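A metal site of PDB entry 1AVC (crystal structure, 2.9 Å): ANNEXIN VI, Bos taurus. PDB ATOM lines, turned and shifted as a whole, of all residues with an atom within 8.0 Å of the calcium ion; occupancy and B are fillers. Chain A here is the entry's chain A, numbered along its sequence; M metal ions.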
ATOM      1  N   ARG A 373     -13.414  10.988  -3.346  1.00  0.00           N
ATOM      2  CA  ARG A 373     -12.862  11.050  -4.697  1.00  0.00           C
ATOM      3  C   ARG A 373     -11.337  10.971  -4.661  1.00  0.00           C
ATOM      4  O   ARG A 373     -10.719  10.295  -5.492  1.00  0.00           O
ATOM      5  CB  ARG A 373     -13.288  12.357  -5.375  1.00  0.00           C
ATOM      6  CG  ARG A 373     -12.513  12.690  -6.634  1.00  0.00           C
ATOM      7  CD  ARG A 373     -13.261  12.232  -7.882  1.00  0.00           C
ATOM      8  NE  ARG A 373     -12.465  12.405  -9.088  1.00  0.00           N
ATOM      9  CZ  ARG A 373     -12.640  11.707 -10.206  1.00  0.00           C
ATOM     10  NH1 ARG A 373     -13.587  10.770 -10.264  1.00  0.00           N
ATOM     11  NH2 ARG A 373     -11.872  11.930 -11.266  1.00  0.00           N
ATOM     12  N   LYS A 374     -10.736  11.645  -3.683  1.00  0.00           N
ATOM     13  CA  LYS A 374      -9.297  11.657  -3.525  1.00  0.00           C
ATOM     14  C   LYS A 374      -8.752  10.278  -3.155  1.00  0.00           C
ATOM     15  O   LYS A 374      -7.734   9.835  -3.695  1.00  0.00           O
ATOM     16  CB  LYS A 374      -8.894  12.666  -2.446  1.00  0.00           C
ATOM     17  CG  LYS A 374      -7.407  12.682  -2.098  1.00  0.00           C
ATOM     18  CD  LYS A 374      -7.087  11.711  -0.957  1.00  0.00           C
ATOM     19  CE  LYS A 374      -7.826  12.078   0.321  1.00  0.00           C
ATOM     20  NZ  LYS A 374      -7.619  11.063   1.381  1.00  0.00           N
ATOM     21  N   ALA A 375      -9.432   9.600  -2.235  1.00  0.00           N
ATOM     22  CA  ALA A 375      -9.014   8.286  -1.769  1.00  0.00           C
ATOM     23  C   ALA A 375      -9.255   7.163  -2.776  1.00  0.00           C
ATOM     24  O   ALA A 375      -9.000   5.996  -2.476  1.00  0.00           O
ATOM     25  CB  ALA A 375      -9.716   7.958  -0.460  1.00  0.00           C
ATOM     26  N   MET A 376      -9.731   7.501  -3.969  1.00  0.00           N
ATOM     27  CA  MET A 376      -9.993   6.501  -4.987  1.00  0.00           C
ATOM     28  C   MET A 376      -9.133   6.709  -6.230  1.00  0.00           C
ATOM     29  O   MET A 376      -8.998   5.816  -7.066  1.00  0.00           O
ATOM     30  CB  MET A 376     -11.474   6.515  -5.376  1.00  0.00           C
ATOM     31  CG  MET A 376     -12.402   5.987  -4.295  1.00  0.00           C
ATOM     32  SD  MET A 376     -14.088   5.761  -4.879  1.00  0.00           S
ATOM     33  CE  MET A 376     -14.860   7.258  -4.298  1.00  0.00           C
ATOM     34  N   LYS A 377      -8.547   7.902  -6.345  1.00  0.00           N
ATOM     35  CA  LYS A 377      -7.705   8.232  -7.488  1.00  0.00           C
ATOM     36  C   LYS A 377      -6.373   7.501  -7.399  1.00  0.00           C
ATOM     37  O   LYS A 377      -5.870   7.230  -6.300  1.00  0.00           O
ATOM     38  CB  LYS A 377      -7.466   9.737  -7.547  1.00  0.00           C
ATOM     39  CG  LYS A 377      -8.228  10.443  -8.654  1.00  0.00           C
ATOM     40  CD  LYS A 377      -9.131  11.540  -8.095  1.00  0.00           C
ATOM     41  CE  LYS A 377      -8.933  12.850  -8.844  1.00  0.00           C
ATOM     42  NZ  LYS A 377      -8.921  14.023  -7.919  1.00  0.00           N
ATOM     43  N   GLY A 378      -5.787   7.187  -8.555  1.00  0.00           N
ATOM     44  CA  GLY A 378      -4.516   6.487  -8.592  1.00  0.00           C
ATOM     45  C   GLY A 378      -4.739   5.011  -8.842  1.00  0.00           C
ATOM     46  O   GLY A 378      -5.851   4.592  -9.151  1.00  0.00           O
ATOM     47  N   LEU A 379      -3.682   4.205  -8.713  1.00  0.00           N
ATOM     48  CA  LEU A 379      -3.822   2.767  -8.916  1.00  0.00           C
ATOM     49  C   LEU A 379      -4.491   2.156  -7.691  1.00  0.00           C
ATOM     50  O   LEU A 379      -5.566   1.556  -7.802  1.00  0.00           O
ATOM     51  CB  LEU A 379      -2.449   2.112  -9.132  1.00  0.00           C
ATOM     52  CG  LEU A 379      -2.512   0.670  -9.656  1.00  0.00           C
ATOM     53  CD1 LEU A 379      -3.189   0.653 -11.017  1.00  0.00           C
ATOM     54  CD2 LEU A 379      -1.119   0.083  -9.741  1.00  0.00           C
ATOM     55  N   GLY A 380      -3.846   2.313  -6.543  1.00  0.00           N
ATOM     56  CA  GLY A 380      -4.381   1.794  -5.301  1.00  0.00           C
ATOM     57  C   GLY A 380      -5.527   2.642  -4.798  1.00  0.00           C
ATOM     58  O   GLY A 380      -5.709   3.783  -5.232  1.00  0.00           O
ATOM     59  N   THR A 381      -6.304   2.102  -3.868  1.00  0.00           N
ATOM     60  CA  THR A 381      -7.443   2.819  -3.312  1.00  0.00           C
ATOM     61  C   THR A 381      -7.305   3.020  -1.808  1.00  0.00           C
ATOM     62  O   THR A 381      -7.232   2.054  -1.052  1.00  0.00           O
ATOM     63  CB  THR A 381      -8.754   2.053  -3.600  1.00  0.00           C
ATOM     64  OG1 THR A 381      -9.647   2.190  -2.488  1.00  0.00           O
ATOM     65  CG2 THR A 381      -8.459   0.583  -3.831  1.00  0.00           C
ATOM     66  N   ASP A 382      -7.270   4.273  -1.374  1.00  0.00           N
ATOM     67  CA  ASP A 382      -7.147   4.592   0.048  1.00  0.00           C
ATOM     68  C   ASP A 382      -8.447   4.165   0.733  1.00  0.00           C
ATOM     69  O   ASP A 382      -9.417   4.911   0.777  1.00  0.00           O
ATOM     70  CB  ASP A 382      -6.935   6.090   0.233  1.00  0.00           C
ATOM     71  CG  ASP A 382      -6.889   6.506   1.697  1.00  0.00           C
ATOM     72  OD1 ASP A 382      -6.999   5.621   2.572  1.00  0.00           O
ATOM     73  OD2 ASP A 382      -6.750   7.718   1.961  1.00  0.00           O
ATOM     74  N   SER A 419     -16.173  -0.397  -8.100  1.00  0.00           N
ATOM     75  CA  SER A 419     -14.979  -0.699  -8.893  1.00  0.00           C
ATOM     76  C   SER A 419     -13.662  -0.587  -8.126  1.00  0.00           C
ATOM     77  O   SER A 419     -12.753  -1.392  -8.340  1.00  0.00           O
ATOM     78  CB  SER A 419     -14.934   0.207 -10.120  1.00  0.00           C
ATOM     79  OG  SER A 419     -13.647   0.752 -10.317  1.00  0.00           O
ATOM     80  N   GLU A 420     -13.551   0.401  -7.245  1.00  0.00           N
ATOM     81  CA  GLU A 420     -12.324   0.597  -6.488  1.00  0.00           C
ATOM     82  C   GLU A 420     -12.219  -0.297  -5.249  1.00  0.00           C
ATOM     83  O   GLU A 420     -11.131  -0.487  -4.701  1.00  0.00           O
ATOM     84  CB  GLU A 420     -12.188   2.061  -6.107  1.00  0.00           C
ATOM     85  CG  GLU A 420     -11.664   2.902  -7.239  1.00  0.00           C
ATOM     86  CD  GLU A 420     -10.160   2.824  -7.316  1.00  0.00           C
ATOM     87  OE1 GLU A 420      -9.521   3.058  -6.278  1.00  0.00           O
ATOM     88  OE2 GLU A 420      -9.625   2.523  -8.396  1.00  0.00           O
ATOM     89  N   LEU A 421     -13.351  -0.844  -4.810  1.00  0.00           N
ATOM     90  CA  LEU A 421     -13.358  -1.726  -3.638  1.00  0.00           C
ATOM     91  C   LEU A 421     -13.623  -3.169  -4.054  1.00  0.00           C
ATOM     92  O   LEU A 421     -14.152  -3.426  -5.141  1.00  0.00           O
ATOM     93  CB  LEU A 421     -14.435  -1.277  -2.651  1.00  0.00           C
ATOM     94  CG  LEU A 421     -14.184   0.026  -1.870  1.00  0.00           C
ATOM     95  CD1 LEU A 421     -15.213   0.154  -0.753  1.00  0.00           C
ATOM     96  CD2 LEU A 421     -12.775   0.019  -1.291  1.00  0.00           C
HETATM   97 CA    CA M   1      -7.204   3.353  -7.125  1.00  0.00          CA
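The calcium ion is bound by the backbone carbonyl oxygen (O) of Gly 380 (2.5 Å), the side-chain carboxylate (OE1) of Glu 420 (2.5 Å), the backbone carbonyl oxygen (O) of Leu 379 (2.5 Å), the backbone carbonyl oxygen (O) of Gly 378 (2.7 Å) and the side-chain carboxylate (OE2) of Glu 420 (2.9 Å).
Slightly farther from the calcium ion lies the backbone carbonyl oxygen (O) of Met 376 (3.0 Å).
Residues that only touch the calcium ion: Thr 381 (3.6 Å).
Six residues have an atom within 4 Å of the calcium ion: Met 376, Gly 378, Leu 379, Gly 380, Thr 381 and Glu 420.
Along chain A the residues within 4 Å of the calcium ion span positions 376 to 420.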
